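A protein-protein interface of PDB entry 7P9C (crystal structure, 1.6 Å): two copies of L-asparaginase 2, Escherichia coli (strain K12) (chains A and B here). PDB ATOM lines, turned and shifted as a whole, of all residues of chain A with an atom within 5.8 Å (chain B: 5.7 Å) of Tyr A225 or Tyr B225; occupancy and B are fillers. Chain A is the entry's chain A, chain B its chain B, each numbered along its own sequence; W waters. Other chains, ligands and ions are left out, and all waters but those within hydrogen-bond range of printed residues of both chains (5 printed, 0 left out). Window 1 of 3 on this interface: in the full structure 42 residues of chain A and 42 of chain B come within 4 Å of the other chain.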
ATOM      1  N   ILE A 223     -10.947  11.275  -9.035  1.00  0.00           N
ATOM      2  CA  ILE A 223     -10.257  11.439 -10.316  1.00  0.00           C
ATOM      3  C   ILE A 223      -9.276  12.602 -10.220  1.00  0.00           C
ATOM      4  O   ILE A 223      -9.635  13.697  -9.767  1.00  0.00           O
ATOM      5  CB  ILE A 223     -11.244  11.675 -11.476  1.00  0.00           C
ATOM      6  CG1 ILE A 223     -12.269  10.542 -11.555  1.00  0.00           C
ATOM      7  CG2 ILE A 223     -10.500  11.850 -12.818  1.00  0.00           C
ATOM      8  CD1 ILE A 223     -13.385  10.785 -12.581  1.00  0.00           C
ATOM      9  N   VAL A 224      -8.052  12.375 -10.679  1.00  0.00           N
ATOM     10  CA  VAL A 224      -7.034  13.418 -10.748  1.00  0.00           C
ATOM     11  C   VAL A 224      -6.595  13.626 -12.194  1.00  0.00           C
ATOM     12  O   VAL A 224      -6.488  12.675 -12.974  1.00  0.00           O
ATOM     13  CB  VAL A 224      -5.822  13.078  -9.866  1.00  0.00           C
ATOM     14  CG1 VAL A 224      -6.258  12.954  -8.421  1.00  0.00           C
ATOM     15  CG2 VAL A 224      -5.147  11.829 -10.309  1.00  0.00           C
ATOM     16  N   TYR A 225      -6.321  14.871 -12.541  1.00  0.00           N
ATOM     17  CA  TYR A 225      -5.922  15.272 -13.882  1.00  0.00           C
ATOM     18  C   TYR A 225      -4.406  15.374 -14.009  1.00  0.00           C
ATOM     19  O   TYR A 225      -3.710  15.774 -13.071  1.00  0.00           O
ATOM     20  CB  TYR A 225      -6.553  16.630 -14.208  1.00  0.00           C
ATOM     21  CG  TYR A 225      -6.871  16.869 -15.676  1.00  0.00           C
ATOM     22  CD1 TYR A 225      -7.887  16.170 -16.298  1.00  0.00           C
ATOM     23  CD2 TYR A 225      -6.161  17.814 -16.432  1.00  0.00           C
ATOM     24  CE1 TYR A 225      -8.211  16.393 -17.622  1.00  0.00           C
ATOM     25  CE2 TYR A 225      -6.476  18.053 -17.779  1.00  0.00           C
ATOM     26  CZ  TYR A 225      -7.520  17.338 -18.363  1.00  0.00           C
ATOM     27  OH  TYR A 225      -7.934  17.533 -19.683  1.00  0.00           O
ATOM     28  N   ASN A 226      -3.901  15.028 -15.190  1.00  0.00           N
ATOM     29  CA  ASN A 226      -2.493  15.199 -15.514  1.00  0.00           C
ATOM     30  C   ASN A 226      -2.325  16.252 -16.610  1.00  0.00           C
ATOM     31  O   ASN A 226      -3.157  16.388 -17.516  1.00  0.00           O
ATOM     32  CB  ASN A 226      -1.828  13.899 -15.980  1.00  0.00           C
ATOM     33  CG  ASN A 226      -1.675  12.873 -14.858  1.00  0.00           C
ATOM     34  OD1 ASN A 226      -0.588  12.699 -14.289  1.00  0.00           O
ATOM     35  ND2 ASN A 226      -2.772  12.195 -14.535  1.00  0.00           N
ATOM     36  N   TYR A 227      -1.216  16.983 -16.513  1.00  0.00           N
ATOM     37  CA  TYR A 227      -0.882  18.113 -17.370  1.00  0.00           C
ATOM     38  C   TYR A 227       0.560  18.502 -17.010  1.00  0.00           C
ATOM     39  O   TYR A 227       1.144  17.975 -16.059  1.00  0.00           O
ATOM     40  CB  TYR A 227      -1.894  19.256 -17.171  1.00  0.00           C
ATOM     41  CG  TYR A 227      -2.087  19.648 -15.721  1.00  0.00           C
ATOM     42  CD1 TYR A 227      -2.909  18.909 -14.885  1.00  0.00           C
ATOM     43  CD2 TYR A 227      -1.414  20.727 -15.182  1.00  0.00           C
ATOM     44  CE1 TYR A 227      -3.071  19.235 -13.566  1.00  0.00           C
ATOM     45  CE2 TYR A 227      -1.591  21.083 -13.868  1.00  0.00           C
ATOM     46  CZ  TYR A 227      -2.429  20.338 -13.061  1.00  0.00           C
ATOM     47  OH  TYR A 227      -2.608  20.642 -11.723  1.00  0.00           O
ATOM     48  N   ALA A 230       2.049  19.309 -13.220  1.00  0.00           N
ATOM     49  CA  ALA A 230       0.909  18.988 -12.369  1.00  0.00           C
ATOM     50  C   ALA A 230       1.279  18.805 -10.901  1.00  0.00           C
ATOM     51  O   ALA A 230       2.277  18.160 -10.557  1.00  0.00           O
ATOM     52  CB  ALA A 230       0.228  17.719 -12.881  1.00  0.00           C
ATOM     53  N   SER A 231       0.451  19.379 -10.032  1.00  0.00           N
ATOM     54  CA  SER A 231       0.650  19.247  -8.593  1.00  0.00           C
ATOM     55  C   SER A 231       0.264  17.845  -8.128  1.00  0.00           C
ATOM     56  O   SER A 231      -0.689  17.253  -8.635  1.00  0.00           O
ATOM     57  CB  SER A 231      -0.198  20.278  -7.846  1.00  0.00           C
ATOM     58  OG  SER A 231      -0.220  20.034  -6.454  1.00  0.00           O
ATOM     59  N   VAL A 247      -8.709   7.236  -9.991  1.00  0.00           N
ATOM     60  CA  VAL A 247      -8.567   7.172 -11.441  1.00  0.00           C
ATOM     61  C   VAL A 247      -7.709   8.344 -11.886  1.00  0.00           C
ATOM     62  O   VAL A 247      -7.988   9.500 -11.533  1.00  0.00           O
ATOM     63  CB  VAL A 247      -9.929   7.217 -12.151  1.00  0.00           C
ATOM     64  CG1 VAL A 247      -9.751   7.330 -13.661  1.00  0.00           C
ATOM     65  CG2 VAL A 247     -10.735   5.995 -11.780  1.00  0.00           C
ATOM     66  N   ALA A 249      -6.619  10.708 -14.920  1.00  0.00           N
ATOM     67  CA  ALA A 249      -6.850  11.193 -16.290  1.00  0.00           C
ATOM     68  C   ALA A 249      -5.489  11.563 -16.841  1.00  0.00           C
ATOM     69  O   ALA A 249      -5.051  12.707 -16.730  1.00  0.00           O
ATOM     70  CB  ALA A 249      -7.790  12.383 -16.337  1.00  0.00           C
ATOM     71  N   VAL A 260       2.723  13.134  -9.746  1.00  0.00           N
ATOM     72  CA  VAL A 260       1.495  12.362  -9.611  1.00  0.00           C
ATOM     73  C   VAL A 260       1.806  10.870  -9.617  1.00  0.00           C
ATOM     74  O   VAL A 260       1.257  10.101  -8.828  1.00  0.00           O
ATOM     75  CB  VAL A 260       0.532  12.751 -10.747  1.00  0.00           C
ATOM     76  CG1 VAL A 260      -0.743  11.909 -10.700  1.00  0.00           C
ATOM     77  CG2 VAL A 260       0.185  14.255 -10.688  1.00  0.00           C
ATOM     78  N   ARG A 279      -6.978  11.664 -20.335  1.00  0.00           N
ATOM     79  CA  ARG A 279      -7.724  12.855 -20.717  1.00  0.00           C
ATOM     80  C   ARG A 279      -7.993  12.924 -22.227  1.00  0.00           C
ATOM     81  O   ARG A 279      -8.789  13.770 -22.661  1.00  0.00           O
ATOM     82  CB  ARG A 279      -6.977  14.132 -20.285  1.00  0.00           C
ATOM     83  CG  ARG A 279      -5.771  14.448 -21.174  1.00  0.00           C
ATOM     84  CD  ARG A 279      -4.884  15.556 -20.630  1.00  0.00           C
ATOM     85  NE  ARG A 279      -3.944  16.040 -21.644  1.00  0.00           N
ATOM     86  CZ  ARG A 279      -3.077  17.022 -21.440  1.00  0.00           C
ATOM     87  NH1 ARG A 279      -2.954  17.589 -20.257  1.00  0.00           N
ATOM     88  NH2 ARG A 279      -2.328  17.450 -22.453  1.00  0.00           N
ATOM     89  N   ASN A 305     -13.114   6.298 -20.481  1.00  0.00           N
ATOM     90  CA  ASN A 305     -12.600   7.608 -20.093  1.00  0.00           C
ATOM     91  C   ASN A 305     -12.654   7.749 -18.564  1.00  0.00           C
ATOM     92  O   ASN A 305     -13.078   6.838 -17.850  1.00  0.00           O
ATOM     93  CB  ASN A 305     -13.362   8.715 -20.835  1.00  0.00           C
ATOM     94  CG  ASN A 305     -14.806   8.866 -20.402  1.00  0.00           C
ATOM     95  OD1 ASN A 305     -15.179   8.607 -19.267  1.00  0.00           O
ATOM     96  ND2 ASN A 305     -15.631   9.313 -21.331  1.00  0.00           N
ATOM     97  N   PRO A 306     -12.113   8.828 -18.015  1.00  0.00           N
ATOM     98  CA  PRO A 306     -11.909   8.837 -16.557  1.00  0.00           C
ATOM     99  C   PRO A 306     -13.199   8.659 -15.763  1.00  0.00           C
ATOM    100  O   PRO A 306     -13.236   7.859 -14.803  1.00  0.00           O
ATOM    101  CB  PRO A 306     -11.223  10.198 -16.340  1.00  0.00           C
ATOM    102  CG  PRO A 306     -10.456  10.439 -17.640  1.00  0.00           C
ATOM    103  CD  PRO A 306     -11.458   9.988 -18.668  1.00  0.00           C
ATOM    104  N   GLN A 307     -14.270   9.382 -16.125  1.00  0.00           N
ATOM    105  CA  GLN A 307     -15.506   9.274 -15.367  1.00  0.00           C
ATOM    106  C   GLN A 307     -16.158   7.914 -15.550  1.00  0.00           C
ATOM    107  O   GLN A 307     -16.842   7.442 -14.642  1.00  0.00           O
ATOM    108  CB  GLN A 307     -16.458  10.401 -15.745  1.00  0.00           C
ATOM    109  CG  GLN A 307     -16.810  10.580 -17.251  1.00  0.00           C
ATOM    110  CD  GLN A 307     -15.825  11.470 -18.021  1.00  0.00           C
ATOM    111  OE1 GLN A 307     -14.685  11.687 -17.597  1.00  0.00           O
ATOM    112  NE2 GLN A 307     -16.282  12.003 -19.168  1.00  0.00           N
ATOM    113  N   ILE B 223      -5.428  22.139 -11.884  1.00  0.00           N
ATOM    114  CA  ILE B 223      -6.636  21.700 -12.589  1.00  0.00           C
ATOM    115  C   ILE B 223      -7.374  20.672 -11.742  1.00  0.00           C
ATOM    116  O   ILE B 223      -6.759  19.711 -11.288  1.00  0.00           O
ATOM    117  CB  ILE B 223      -6.296  21.086 -13.959  1.00  0.00           C
ATOM    118  CG1 ILE B 223      -5.536  22.114 -14.817  1.00  0.00           C
ATOM    119  CG2 ILE B 223      -7.588  20.628 -14.674  1.00  0.00           C
ATOM    120  CD1 ILE B 223      -5.123  21.664 -16.213  1.00  0.00           C
ATOM    121  N   VAL B 224      -8.684  20.854 -11.548  1.00  0.00           N
ATOM    122  CA  VAL B 224      -9.524  19.859 -10.875  1.00  0.00           C
ATOM    123  C   VAL B 224     -10.607  19.342 -11.815  1.00  0.00           C
ATOM    124  O   VAL B 224     -11.168  20.102 -12.605  1.00  0.00           O
ATOM    125  CB  VAL B 224     -10.168  20.436  -9.601  1.00  0.00           C
ATOM    126  CG1 VAL B 224      -9.081  20.789  -8.562  1.00  0.00           C
ATOM    127  CG2 VAL B 224     -11.018  21.657  -9.893  1.00  0.00           C
ATOM    128  N   TYR B 225     -10.947  18.060 -11.688  1.00  0.00           N
ATOM    129  CA  TYR B 225     -11.933  17.399 -12.534  1.00  0.00           C
ATOM    130  C   TYR B 225     -13.298  17.377 -11.858  1.00  0.00           C
ATOM    131  O   TYR B 225     -13.388  17.210 -10.640  1.00  0.00           O
ATOM    132  CB  TYR B 225     -11.458  15.965 -12.819  1.00  0.00           C
ATOM    133  CG  TYR B 225     -11.872  15.366 -14.144  1.00  0.00           C
ATOM    134  CD1 TYR B 225     -11.303  15.790 -15.331  1.00  0.00           C
ATOM    135  CD2 TYR B 225     -12.808  14.341 -14.208  1.00  0.00           C
ATOM    136  CE1 TYR B 225     -11.661  15.234 -16.551  1.00  0.00           C
ATOM    137  CE2 TYR B 225     -13.161  13.777 -15.400  1.00  0.00           C
ATOM    138  CZ  TYR B 225     -12.583  14.229 -16.595  1.00  0.00           C
ATOM    139  OH  TYR B 225     -12.928  13.700 -17.827  1.00  0.00           O
ATOM    140  N   ASN B 226     -14.352  17.485 -12.652  1.00  0.00           N
ATOM    141  CA  ASN B 226     -15.720  17.353 -12.172  1.00  0.00           C
ATOM    142  C   ASN B 226     -16.334  16.085 -12.766  1.00  0.00           C
ATOM    143  O   ASN B 226     -16.020  15.673 -13.892  1.00  0.00           O
ATOM    144  CB  ASN B 226     -16.583  18.572 -12.524  1.00  0.00           C
ATOM    145  CG  ASN B 226     -16.214  19.795 -11.747  1.00  0.00           C
ATOM    146  OD1 ASN B 226     -16.835  20.112 -10.735  1.00  0.00           O
ATOM    147  ND2 ASN B 226     -15.216  20.521 -12.227  1.00  0.00           N
ATOM    148  N   TYR B 227     -17.208  15.472 -11.974  1.00  0.00           N
ATOM    149  CA  TYR B 227     -17.819  14.186 -12.270  1.00  0.00           C
ATOM    150  C   TYR B 227     -18.857  13.957 -11.170  1.00  0.00           C
ATOM    151  O   TYR B 227     -18.961  14.738 -10.215  1.00  0.00           O
ATOM    152  CB  TYR B 227     -16.774  13.074 -12.340  1.00  0.00           C
ATOM    153  CG  TYR B 227     -15.884  12.993 -11.127  1.00  0.00           C
ATOM    154  CD1 TYR B 227     -14.800  13.836 -10.986  1.00  0.00           C
ATOM    155  CD2 TYR B 227     -16.148  12.097 -10.094  1.00  0.00           C
ATOM    156  CE1 TYR B 227     -14.010  13.815  -9.864  1.00  0.00           C
ATOM    157  CE2 TYR B 227     -15.330  12.049  -8.975  1.00  0.00           C
ATOM    158  CZ  TYR B 227     -14.249  12.905  -8.874  1.00  0.00           C
ATOM    159  OH  TYR B 227     -13.407  12.907  -7.764  1.00  0.00           O
ATOM    160  N   ALA B 230     -18.283  14.210  -7.077  1.00  0.00           N
ATOM    161  CA  ALA B 230     -16.893  14.650  -7.022  1.00  0.00           C
ATOM    162  C   ALA B 230     -16.523  15.194  -5.652  1.00  0.00           C
ATOM    163  O   ALA B 230     -17.252  15.984  -5.057  1.00  0.00           O
ATOM    164  CB  ALA B 230     -16.643  15.727  -8.070  1.00  0.00           C
ATOM    165  N   SER B 231     -15.360  14.784  -5.166  1.00  0.00           N
ATOM    166  CA  SER B 231     -14.844  15.301  -3.904  1.00  0.00           C
ATOM    167  C   SER B 231     -14.377  16.746  -4.048  1.00  0.00           C
ATOM    168  O   SER B 231     -13.792  17.118  -5.067  1.00  0.00           O
ATOM    169  CB  SER B 231     -13.671  14.447  -3.451  1.00  0.00           C
ATOM    170  OG  SER B 231     -13.104  14.976  -2.268  1.00  0.00           O
ATOM    171  N   ALA B 249     -12.102  21.591 -14.791  1.00  0.00           N
ATOM    172  CA  ALA B 249     -12.564  20.776 -15.908  1.00  0.00           C
ATOM    173  C   ALA B 249     -13.998  20.393 -15.575  1.00  0.00           C
ATOM    174  O   ALA B 249     -14.264  19.372 -14.954  1.00  0.00           O
ATOM    175  CB  ALA B 249     -11.667  19.564 -16.102  1.00  0.00           C
ATOM    176  N   VAL B 260     -17.535  21.236  -5.222  1.00  0.00           N
ATOM    177  CA  VAL B 260     -16.424  21.892  -5.904  1.00  0.00           C
ATOM    178  C   VAL B 260     -16.758  23.359  -6.141  1.00  0.00           C
ATOM    179  O   VAL B 260     -15.938  24.243  -5.873  1.00  0.00           O
ATOM    180  CB  VAL B 260     -16.099  21.157  -7.222  1.00  0.00           C
ATOM    181  CG1 VAL B 260     -14.965  21.840  -7.953  1.00  0.00           C
ATOM    182  CG2 VAL B 260     -15.762  19.694  -6.952  1.00  0.00           C
ATOM    183  N   ARG B 279     -14.402  19.348 -19.298  1.00  0.00           N
ATOM    184  CA  ARG B 279     -13.889  18.044 -19.694  1.00  0.00           C
ATOM    185  C   ARG B 279     -14.428  17.587 -21.049  1.00  0.00           C
ATOM    186  O   ARG B 279     -13.916  16.613 -21.612  1.00  0.00           O
ATOM    187  CB  ARG B 279     -14.223  17.000 -18.634  1.00  0.00           C
ATOM    188  CG  ARG B 279     -15.658  16.505 -18.737  1.00  0.00           C
ATOM    189  CD  ARG B 279     -16.081  15.631 -17.530  1.00  0.00           C
ATOM    190  NE  ARG B 279     -17.363  15.000 -17.796  1.00  0.00           N
ATOM    191  CZ  ARG B 279     -17.972  14.141 -16.992  1.00  0.00           C
ATOM    192  NH1 ARG B 279     -17.471  13.837 -15.791  1.00  0.00           N
ATOM    193  NH2 ARG B 279     -19.103  13.559 -17.406  1.00  0.00           N
ATOM    194  N   PRO B 306      -9.016  22.294 -20.528  1.00  0.00           N
ATOM    195  CA  PRO B 306      -8.487  22.647 -19.195  1.00  0.00           C
ATOM    196  C   PRO B 306      -6.981  22.926 -19.203  1.00  0.00           C
ATOM    197  O   PRO B 306      -6.519  23.910 -18.599  1.00  0.00           O
ATOM    198  CB  PRO B 306      -8.866  21.421 -18.346  1.00  0.00           C
ATOM    199  CG  PRO B 306     -10.155  20.886 -18.996  1.00  0.00           C
ATOM    200  CD  PRO B 306      -9.795  21.046 -20.493  1.00  0.00           C
ATOM    201  N   GLN B 307      -6.197  22.079 -19.881  1.00  0.00           N
ATOM    202  CA  GLN B 307      -4.755  22.297 -19.898  1.00  0.00           C
ATOM    203  C   GLN B 307      -4.345  23.548 -20.685  1.00  0.00           C
ATOM    204  O   GLN B 307      -3.323  24.177 -20.362  1.00  0.00           O
ATOM    205  CB  GLN B 307      -4.058  21.039 -20.413  1.00  0.00           C
ATOM    206  CG  GLN B 307      -4.433  20.468 -21.754  1.00  0.00           C
ATOM    207  CD  GLN B 307      -5.605  19.503 -21.738  1.00  0.00           C
ATOM    208  OE1 GLN B 307      -6.414  19.480 -20.820  1.00  0.00           O
ATOM    209  NE2 GLN B 307      -5.714  18.713 -22.798  1.00  0.00           N
HETATM  210  O   HOH W   1     -11.753  15.265 -23.326  1.00  0.00           O
HETATM  211  O   HOH W   2     -14.750  13.808 -21.089  1.00  0.00           O
HETATM  212  O   HOH W   3      -7.964  16.696 -23.145  1.00  0.00           O
HETATM  213  O   HOH W   4      -9.361  16.387  -9.682  1.00  0.00           O
HETATM  214  O   HOH W   5      -6.837  17.066 -10.451  1.00  0.00           O
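Hydrophobic or aromatic side chains of chain B within 4 Å of the printed part of chain A: Ile B223, Tyr B225 and Tyr B227.
Of the 14 printed residues of chain A, 5 touch a printed residue of chain B.
Among the printed residues, 9 pairs touch across the chains.
Among the printed residues, no Asp or Glu carboxylate lies within 4 Å of a Lys or Arg side-chain nitrogen of the other chain.
Of chain B, only Ile B223, Tyr B225 and Gln B307 come within 4 Å of Tyr A225.
Tyr B225 touches just these residues of chain A: Ile A223 (3.7 Å), Tyr A225 (3.6 Å) and Gln A307 (2.7 Å).
Of the printed residues of chain A, Gln B307 touches Tyr A225 (2.7 Å) and Arg A279 (3.4 Å).
Of the printed residues of chain B, Ile A223 touches Tyr B225 (3.7 Å) and Tyr B227 (3.2 Å).
The nearest residue of chain A that does not touch Tyr B225 is Pro A306 (4.1 Å).
The nearest printed residue of chain B that does not touch Gln A307 is Tyr B227 (4.3 Å).
Among the printed residues, pairs that only touch across the chains: Ile A223 with Tyr B225, Tyr A225 with Ile B223 and Tyr A225 with Tyr B225.
Ile A223 touches Tyr B225, and with the chains exchanged Tyr A225 touches Ile B223.
Ile A223 touches Tyr B227, and with the chains exchanged Tyr A227 touches Ile B223.
Tyr A225 touches its own counterpart, Tyr B225.
Tyr A225 touches Gln B307, and with the chains exchanged Gln A307 touches Tyr B225.
Of the 9 pairs that touch across the chains among the printed residues, 9 have their exchanged pair printed and touching as well.
The guanidinium group (NH1) of Arg B279 lies within hydrogen-bond range of the backbone carbonyl oxygen (O) of Asn B226 (3.0 Å).
The side-chain amide oxygen (OD1) of Asn A305 lies close to the backbone NH (N) of Gln A307, 3.4 Å away.
O of Asn A226 sits at hydrogen-bond distance from NH1 of Arg A279.
The side-chain amide oxygen (OE1) of Gln A307 sits at hydrogen-bond distance from the side-chain hydroxyl (OH) of Tyr B225 (2.7 Å).
NE of Arg A279 lies close to NE2 of Gln B307 (3.4 Å).
The side-chain amide nitrogen of Gln A307 sits close to the guanidinium group of Arg B279.
The backbone NH of Ile A223 sits at hydrogen-bond distance from the side-chain hydroxyl of Tyr B227, 3.2 Å away.
The side-chain amide oxygen (OE1) of Gln B307 sits at hydrogen-bond distance from the side-chain hydroxyl (OH) of Tyr A225 (2.7 Å).
The backbone NH (N) of Ile B223 sits at hydrogen-bond distance from the side-chain hydroxyl (OH) of Tyr A227, at 3.2 Å.
Water W4 bridges the backbone carbonyl oxygen of Ile A223 (2.7 Å) and the backbone NH of Tyr B225 (3.1 Å).
Water W5 bridges the backbone carbonyl oxygen of Ile B223 and the backbone NH of Tyr A225.
Water W2 lies within hydrogen-bond range of O of Arg B279 (3.0 Å) and NE2 of Gln A307 (3.0 Å).
Water W3 bridges the side-chain amide nitrogen (NE2) of Gln B307 and the backbone carbonyl oxygen (O) of Arg A279.
Water W1 lies within hydrogen-bond range of O of Arg B279 (3.1 Å) and O of Arg A279 (3.4 Å).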
